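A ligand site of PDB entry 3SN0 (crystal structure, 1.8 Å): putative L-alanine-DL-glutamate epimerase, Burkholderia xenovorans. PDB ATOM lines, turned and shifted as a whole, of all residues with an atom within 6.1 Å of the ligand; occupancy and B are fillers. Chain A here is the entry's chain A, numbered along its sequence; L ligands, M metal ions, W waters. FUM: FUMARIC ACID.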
ATOM      1  N   PHE A  41      -9.340  -7.763   4.508  1.00  0.00           N
ATOM      2  CA  PHE A  41      -9.004  -7.390   3.135  1.00  0.00           C
ATOM      3  C   PHE A  41     -10.018  -7.990   2.161  1.00  0.00           C
ATOM      4  O   PHE A  41      -9.676  -8.755   1.263  1.00  0.00           O
ATOM      5  CB  PHE A  41      -7.567  -7.798   2.817  1.00  0.00           C
ATOM      6  CG  PHE A  41      -6.961  -7.074   1.636  1.00  0.00           C
ATOM      7  CD1 PHE A  41      -6.958  -5.672   1.592  1.00  0.00           C
ATOM      8  CD2 PHE A  41      -6.390  -7.770   0.593  1.00  0.00           C
ATOM      9  CE1 PHE A  41      -6.388  -5.002   0.513  1.00  0.00           C
ATOM     10  CE2 PHE A  41      -5.808  -7.104  -0.492  1.00  0.00           C
ATOM     11  CZ  PHE A  41      -5.807  -5.716  -0.526  1.00  0.00           C
ATOM     12  N   SER A 124       6.921  -2.017   3.736  1.00  0.00           N
ATOM     13  CA  SER A 124       5.645  -1.803   3.059  1.00  0.00           C
ATOM     14  C   SER A 124       4.796  -0.778   3.788  1.00  0.00           C
ATOM     15  O   SER A 124       5.049  -0.445   4.950  1.00  0.00           O
ATOM     16  CB  SER A 124       4.919  -3.142   2.950  1.00  0.00           C
ATOM     17  OG  SER A 124       3.876  -3.053   1.996  1.00  0.00           O
ATOM     18  N   HIS A 125       3.755  -0.289   3.125  1.00  0.00           N
ATOM     19  CA  HIS A 125       2.846   0.687   3.721  1.00  0.00           C
ATOM     20  C   HIS A 125       3.612   1.820   4.398  1.00  0.00           C
ATOM     21  O   HIS A 125       3.385   2.152   5.554  1.00  0.00           O
ATOM     22  CB  HIS A 125       1.881  -0.016   4.676  1.00  0.00           C
ATOM     23  CG  HIS A 125       1.140  -1.142   4.008  1.00  0.00           C
ATOM     24  ND1 HIS A 125       1.535  -2.456   4.136  1.00  0.00           N
ATOM     25  CD2 HIS A 125       0.110  -1.140   3.132  1.00  0.00           C
ATOM     26  CE1 HIS A 125       0.753  -3.212   3.377  1.00  0.00           C
ATOM     27  NE2 HIS A 125      -0.126  -2.440   2.765  1.00  0.00           N
ATOM     28  N   THR A 128       2.198   4.826   4.232  1.00  0.00           N
ATOM     29  CA  THR A 128       0.765   4.544   4.220  1.00  0.00           C
ATOM     30  C   THR A 128       0.153   4.280   5.616  1.00  0.00           C
ATOM     31  O   THR A 128      -0.863   4.850   5.954  1.00  0.00           O
ATOM     32  CB  THR A 128       0.500   3.368   3.308  1.00  0.00           C
ATOM     33  OG1 THR A 128       1.126   3.627   2.036  1.00  0.00           O
ATOM     34  CG2 THR A 128      -0.997   3.106   3.132  1.00  0.00           C
ATOM     35  N   TRP A 129       0.797   3.439   6.425  1.00  0.00           N
ATOM     36  CA  TRP A 129       0.255   3.128   7.751  1.00  0.00           C
ATOM     37  C   TRP A 129       0.307   4.321   8.719  1.00  0.00           C
ATOM     38  O   TRP A 129      -0.604   4.505   9.528  1.00  0.00           O
ATOM     39  CB  TRP A 129       0.991   1.936   8.381  1.00  0.00           C
ATOM     40  CG  TRP A 129       0.561   0.506   7.988  1.00  0.00           C
ATOM     41  CD1 TRP A 129       1.157  -0.639   8.435  1.00  0.00           C
ATOM     42  CD2 TRP A 129      -0.490   0.084   7.101  1.00  0.00           C
ATOM     43  NE1 TRP A 129       0.544  -1.746   7.905  1.00  0.00           N
ATOM     44  CE2 TRP A 129      -0.471  -1.325   7.078  1.00  0.00           C
ATOM     45  CE3 TRP A 129      -1.436   0.753   6.309  1.00  0.00           C
ATOM     46  CZ2 TRP A 129      -1.349  -2.081   6.304  1.00  0.00           C
ATOM     47  CZ3 TRP A 129      -2.317  -0.003   5.544  1.00  0.00           C
ATOM     48  CH2 TRP A 129      -2.267  -1.404   5.555  1.00  0.00           C
ATOM     49  N   ASN A 132      -2.622   6.617   7.358  1.00  0.00           N
ATOM     50  CA  ASN A 132      -3.977   6.077   7.380  1.00  0.00           C
ATOM     51  C   ASN A 132      -4.412   5.530   8.730  1.00  0.00           C
ATOM     52  O   ASN A 132      -5.604   5.561   9.026  1.00  0.00           O
ATOM     53  CB  ASN A 132      -4.165   4.995   6.297  1.00  0.00           C
ATOM     54  CG  ASN A 132      -4.116   5.567   4.903  1.00  0.00           C
ATOM     55  OD1 ASN A 132      -4.204   6.776   4.710  1.00  0.00           O
ATOM     56  ND2 ASN A 132      -4.019   4.687   3.906  1.00  0.00           N
ATOM     57  N   LYS A 163       7.518   0.909   0.101  1.00  0.00           N
ATOM     58  CA  LYS A 163       6.336   0.952  -0.770  1.00  0.00           C
ATOM     59  C   LYS A 163       5.266   1.876  -0.249  1.00  0.00           C
ATOM     60  O   LYS A 163       4.831   1.759   0.909  1.00  0.00           O
ATOM     61  CB  LYS A 163       5.743  -0.437  -0.989  1.00  0.00           C
ATOM     62  CG  LYS A 163       4.717  -0.477  -2.123  1.00  0.00           C
ATOM     63  CD  LYS A 163       4.356  -1.901  -2.554  1.00  0.00           C
ATOM     64  CE  LYS A 163       3.362  -2.560  -1.609  1.00  0.00           C
ATOM     65  NZ  LYS A 163       3.235  -4.014  -1.905  1.00  0.00           N
ATOM     66  N   ASN A 165       1.475   4.188  -1.411  1.00  0.00           N
ATOM     67  CA  ASN A 165       0.184   4.070  -2.147  1.00  0.00           C
ATOM     68  C   ASN A 165      -0.174   5.473  -2.655  1.00  0.00           C
ATOM     69  O   ASN A 165       0.733   6.260  -2.889  1.00  0.00           O
ATOM     70  CB  ASN A 165      -0.892   3.473  -1.211  1.00  0.00           C
ATOM     71  CG  ASN A 165      -0.525   2.080  -0.710  1.00  0.00           C
ATOM     72  OD1 ASN A 165       0.232   1.916   0.260  1.00  0.00           O
ATOM     73  ND2 ASN A 165      -1.098   1.040  -1.362  1.00  0.00           N
ATOM     74  N   ARG A 178      -8.405   6.048  -2.493  1.00  0.00           N
ATOM     75  CA  ARG A 178      -8.679   4.611  -2.567  1.00  0.00           C
ATOM     76  C   ARG A 178     -10.052   4.300  -3.200  1.00  0.00           C
ATOM     77  O   ARG A 178     -10.815   3.510  -2.642  1.00  0.00           O
ATOM     78  CB  ARG A 178      -8.625   4.018  -1.144  1.00  0.00           C
ATOM     79  CG  ARG A 178      -7.269   4.221  -0.424  1.00  0.00           C
ATOM     80  CD  ARG A 178      -7.377   3.940   1.084  1.00  0.00           C
ATOM     81  NE  ARG A 178      -7.737   2.558   1.310  1.00  0.00           N
ATOM     82  CZ  ARG A 178      -8.948   2.125   1.650  1.00  0.00           C
ATOM     83  NH1 ARG A 178      -9.151   0.822   1.769  1.00  0.00           N
ATOM     84  NH2 ARG A 178      -9.970   2.978   1.876  1.00  0.00           N
ATOM     85  N   PHE A 181     -11.518   0.788  -3.523  1.00  0.00           N
ATOM     86  CA  PHE A 181     -12.082   0.242  -2.299  1.00  0.00           C
ATOM     87  C   PHE A 181     -13.154   1.148  -1.704  1.00  0.00           C
ATOM     88  O   PHE A 181     -13.464   1.075  -0.495  1.00  0.00           O
ATOM     89  CB  PHE A 181     -10.954  -0.021  -1.284  1.00  0.00           C
ATOM     90  CG  PHE A 181      -9.899  -1.010  -1.748  1.00  0.00           C
ATOM     91  CD1 PHE A 181     -10.227  -2.141  -2.511  1.00  0.00           C
ATOM     92  CD2 PHE A 181      -8.555  -0.829  -1.376  1.00  0.00           C
ATOM     93  CE1 PHE A 181      -9.238  -3.039  -2.901  1.00  0.00           C
ATOM     94  CE2 PHE A 181      -7.575  -1.721  -1.770  1.00  0.00           C
ATOM     95  CZ  PHE A 181      -7.918  -2.841  -2.539  1.00  0.00           C
ATOM     96  N   ASP A 219       2.312   1.320  -5.131  1.00  0.00           N
ATOM     97  CA  ASP A 219       1.168   0.420  -5.252  1.00  0.00           C
ATOM     98  C   ASP A 219      -0.082   1.230  -5.579  1.00  0.00           C
ATOM     99  O   ASP A 219      -0.500   2.082  -4.794  1.00  0.00           O
ATOM    100  CB  ASP A 219       0.987  -0.381  -3.960  1.00  0.00           C
ATOM    101  CG  ASP A 219       0.162  -1.630  -4.148  1.00  0.00           C
ATOM    102  OD1 ASP A 219      -0.669  -1.668  -5.088  1.00  0.00           O
ATOM    103  OD2 ASP A 219       0.338  -2.577  -3.333  1.00  0.00           O
ATOM    104  N   ASN A 221      -2.959  -0.463  -6.359  1.00  0.00           N
ATOM    105  CA  ASN A 221      -4.038  -1.408  -6.090  1.00  0.00           C
ATOM    106  C   ASN A 221      -5.037  -1.488  -7.269  1.00  0.00           C
ATOM    107  O   ASN A 221      -4.620  -1.621  -8.431  1.00  0.00           O
ATOM    108  CB  ASN A 221      -4.695  -1.076  -4.737  1.00  0.00           C
ATOM    109  CG  ASN A 221      -3.707  -1.051  -3.596  1.00  0.00           C
ATOM    110  OD1 ASN A 221      -3.170  -0.007  -3.248  1.00  0.00           O
ATOM    111  ND2 ASN A 221      -3.443  -2.216  -3.011  1.00  0.00           N
ATOM    112  N   ASN A 223      -7.123   0.990  -8.037  1.00  0.00           N
ATOM    113  CA  ASN A 223      -7.657   2.369  -8.013  1.00  0.00           C
ATOM    114  C   ASN A 223      -7.825   3.101  -9.347  1.00  0.00           C
ATOM    115  O   ASN A 223      -8.093   4.310  -9.363  1.00  0.00           O
ATOM    116  CB  ASN A 223      -6.799   3.218  -7.049  1.00  0.00           C
ATOM    117  CG  ASN A 223      -7.000   2.797  -5.615  1.00  0.00           C
ATOM    118  OD1 ASN A 223      -8.136   2.558  -5.186  1.00  0.00           O
ATOM    119  ND2 ASN A 223      -5.911   2.706  -4.857  1.00  0.00           N
ATOM    120  N   GLU A 245       2.778  -1.368  -8.885  1.00  0.00           N
ATOM    121  CA  GLU A 245       1.919  -2.489  -8.577  1.00  0.00           C
ATOM    122  C   GLU A 245       0.481  -2.148  -8.959  1.00  0.00           C
ATOM    123  O   GLU A 245      -0.051  -1.129  -8.515  1.00  0.00           O
ATOM    124  CB  GLU A 245       2.020  -2.784  -7.074  1.00  0.00           C
ATOM    125  CG  GLU A 245       1.588  -4.169  -6.628  1.00  0.00           C
ATOM    126  CD  GLU A 245       1.954  -4.454  -5.171  1.00  0.00           C
ATOM    127  OE1 GLU A 245       1.167  -5.180  -4.534  1.00  0.00           O
ATOM    128  OE2 GLU A 245       2.995  -3.961  -4.673  1.00  0.00           O
ATOM    129  N   GLU A 269      -1.475 -10.270  -6.417  1.00  0.00           N
ATOM    130  CA  GLU A 269      -1.612 -10.562  -4.985  1.00  0.00           C
ATOM    131  C   GLU A 269      -2.957 -11.158  -4.585  1.00  0.00           C
ATOM    132  O   GLU A 269      -3.066 -11.723  -3.494  1.00  0.00           O
ATOM    133  CB  GLU A 269      -1.340  -9.329  -4.123  1.00  0.00           C
ATOM    134  CG  GLU A 269      -2.483  -8.309  -4.080  1.00  0.00           C
ATOM    135  CD  GLU A 269      -2.096  -7.011  -3.407  1.00  0.00           C
ATOM    136  OE1 GLU A 269      -2.951  -6.422  -2.682  1.00  0.00           O
ATOM    137  OE2 GLU A 269      -0.938  -6.580  -3.574  1.00  0.00           O
ATOM    138  N   HIS A 318       3.055 -11.847  -0.430  1.00  0.00           N
ATOM    139  CA  HIS A 318       2.189 -10.802   0.077  1.00  0.00           C
ATOM    140  C   HIS A 318       2.206 -10.934   1.595  1.00  0.00           C
ATOM    141  O   HIS A 318       1.784 -11.934   2.142  1.00  0.00           O
ATOM    142  CB  HIS A 318       0.786 -11.034  -0.469  1.00  0.00           C
ATOM    143  CG  HIS A 318      -0.107  -9.831  -0.419  1.00  0.00           C
ATOM    144  ND1 HIS A 318      -1.470  -9.935  -0.495  1.00  0.00           N
ATOM    145  CD2 HIS A 318       0.175  -8.503  -0.399  1.00  0.00           C
ATOM    146  CE1 HIS A 318      -2.007  -8.731  -0.477  1.00  0.00           C
ATOM    147  NE2 HIS A 318      -1.028  -7.841  -0.444  1.00  0.00           N
ATOM    148  N   PHE A 320       1.642  -8.522   5.033  1.00  0.00           N
ATOM    149  CA  PHE A 320       1.291  -7.245   5.674  1.00  0.00           C
ATOM    150  C   PHE A 320       0.343  -7.469   6.854  1.00  0.00           C
ATOM    151  O   PHE A 320      -0.560  -6.683   7.113  1.00  0.00           O
ATOM    152  CB  PHE A 320       0.676  -6.272   4.655  1.00  0.00           C
ATOM    153  CG  PHE A 320      -0.655  -6.707   4.088  1.00  0.00           C
ATOM    154  CD1 PHE A 320      -1.809  -5.969   4.323  1.00  0.00           C
ATOM    155  CD2 PHE A 320      -0.742  -7.806   3.248  1.00  0.00           C
ATOM    156  CE1 PHE A 320      -3.042  -6.375   3.784  1.00  0.00           C
ATOM    157  CE2 PHE A 320      -1.970  -8.217   2.722  1.00  0.00           C
ATOM    158  CZ  PHE A 320      -3.108  -7.496   2.984  1.00  0.00           C
ATOM    159  N   GLU A 343       7.971  -8.613   1.055  1.00  0.00           N
ATOM    160  CA  GLU A 343       7.255  -7.522   1.687  1.00  0.00           C
ATOM    161  C   GLU A 343       7.243  -7.726   3.181  1.00  0.00           C
ATOM    162  O   GLU A 343       7.124  -8.854   3.671  1.00  0.00           O
ATOM    163  CB  GLU A 343       5.809  -7.529   1.195  1.00  0.00           C
ATOM    164  CG  GLU A 343       4.964  -6.424   1.787  1.00  0.00           C
ATOM    165  CD  GLU A 343       3.519  -6.462   1.370  1.00  0.00           C
ATOM    166  OE1 GLU A 343       3.044  -7.496   0.842  1.00  0.00           O
ATOM    167  OE2 GLU A 343       2.853  -5.448   1.589  1.00  0.00           O
ATOM    168  N   LEU A 395     -10.977  -3.225   5.040  1.00  0.00           N
ATOM    169  CA  LEU A 395     -11.644  -2.378   4.029  1.00  0.00           C
ATOM    170  C   LEU A 395     -12.965  -1.777   4.528  1.00  0.00           C
ATOM    171  O   LEU A 395     -13.368  -0.685   4.079  1.00  0.00           O
ATOM    172  CB  LEU A 395     -11.860  -3.132   2.708  1.00  0.00           C
ATOM    173  CG  LEU A 395     -10.584  -3.679   2.054  1.00  0.00           C
ATOM    174  CD1 LEU A 395     -10.912  -4.399   0.722  1.00  0.00           C
ATOM    175  CD2 LEU A 395      -9.522  -2.583   1.836  1.00  0.00           C
ATOM    176  N   TYR A 398     -12.212   1.748   6.925  1.00  0.00           N
ATOM    177  CA  TYR A 398     -11.885   2.993   6.197  1.00  0.00           C
ATOM    178  C   TYR A 398     -13.185   3.706   5.858  1.00  0.00           C
ATOM    179  O   TYR A 398     -13.279   4.934   5.922  1.00  0.00           O
ATOM    180  CB  TYR A 398     -11.151   2.723   4.887  1.00  0.00           C
ATOM    181  CG  TYR A 398      -9.749   2.179   4.991  1.00  0.00           C
ATOM    182  CD1 TYR A 398      -8.640   3.026   5.075  1.00  0.00           C
ATOM    183  CD2 TYR A 398      -9.514   0.809   4.969  1.00  0.00           C
ATOM    184  CE1 TYR A 398      -7.346   2.530   5.149  1.00  0.00           C
ATOM    185  CE2 TYR A 398      -8.234   0.295   5.047  1.00  0.00           C
ATOM    186  CZ  TYR A 398      -7.148   1.153   5.144  1.00  0.00           C
ATOM    187  OH  TYR A 398      -5.883   0.650   5.217  1.00  0.00           O
HETATM  188  OXT FUM L   1      -5.734   0.825   0.230  1.00  0.00           O
HETATM  189  C   FUM L   1      -5.752  -0.243   0.901  1.00  0.00           C
HETATM  190  O   FUM L   1      -6.760  -0.534   1.604  1.00  0.00           O
HETATM  191  C4  FUM L   1      -4.601  -1.169   0.939  1.00  0.00           C
HETATM  192  C5  FUM L   1      -3.486  -0.950   0.222  1.00  0.00           C
HETATM  193  C6  FUM L   1      -2.353  -1.903   0.263  1.00  0.00           C
HETATM  194  O7  FUM L   1      -2.409  -2.877   1.072  1.00  0.00           O
HETATM  195  O8  FUM L   1      -1.371  -1.722  -0.507  1.00  0.00           O
HETATM  196 MG    MG M   1      -0.323  -4.655  -3.448  1.00  0.00          MG
HETATM  197  O   HOH W   1      -1.535  -4.257  -1.913  1.00  0.00           O
HETATM  198  O   HOH W   2      -3.716   2.483   1.038  1.00  0.00           O
HETATM  199  O   HOH W   3      -5.570   1.585  -2.284  1.00  0.00           O
HETATM  200  O   HOH W   4      -6.260  -1.865   3.943  1.00  0.00           O
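NH1 of Arg 178 lies within salt-bridge range of O of the ligand, 2.8 Å away.
An oxygen (O7) of the ligand lies within hydrogen-bond range of a ring nitrogen (NE2) of His 125, 2.9 Å away.
An oxygen (O8) of the ligand sits at hydrogen-bond distance from the side-chain amide nitrogen (ND2) of Asn 165, at 2.9 Å.
ND2 of Asn 221 sits at hydrogen-bond distance from O8 of the ligand (3.3 Å).
O8 of the ligand lies close to OD2 of Asp 219, 3.4 Å away.
Phe 181 touches the ligand (CD2 to O, 3.5 Å).
Leu 395 touches the ligand (CD2 to O, 3.4 Å).
Tyr 398 touches the ligand.
Hydrophobic or aromatic side chains that line the ligand: His 125, Phe 181, Leu 395 and Tyr 398.
Eight residues have an atom within 4 Å of the ligand: His 125, Asn 165, Arg 178, Phe 181, Asp 219, Asn 221, Leu 395 and Tyr 398.
Water W3 lies within hydrogen-bond range of an oxygen (OXT) of the ligand (2.6 Å), the side-chain amide nitrogen of Asn 223 (2.8 Å) and the side-chain amide oxygen of Asn 221 (3.0 Å).
Water W4 bridges an oxygen (O) of the ligand (2.7 Å) and the side-chain hydroxyl (OH) of Tyr 398 (2.8 Å).
Water W1 lies within hydrogen-bond range of the side-chain carboxylate (OE1) of Glu 269 (2.7 Å), an oxygen (O8) of the ligand (2.9 Å) and the side-chain amide nitrogen (ND2) of Asn 221 (3.0 Å).
The backbone carbonyl oxygen of Lys 163 sits at hydrogen-bond distance from the backbone NH of His 125 (3.2 Å).
A ring nitrogen (ND1) of His 125 lies within hydrogen-bond range of the side-chain hydroxyl of Ser 124 (3.2 Å).
The side-chain amide nitrogen (ND2) of Asn 165 is in hydrogen-bond range of the side-chain amide oxygen (OD1) of Asn 221 (3.0 Å).
The side-chain amide oxygen of Asn 165 is in hydrogen-bond range of the side-chain hydroxyl of Thr 128 (2.6 Å).
The backbone NH (N) of Asn 221 lies within hydrogen-bond range of the side-chain carboxylate (OD1) of Asp 219, at 2.9 Å.
NZ of Lys 163 sits close to OD2 of Asp 219 (3.5 Å).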
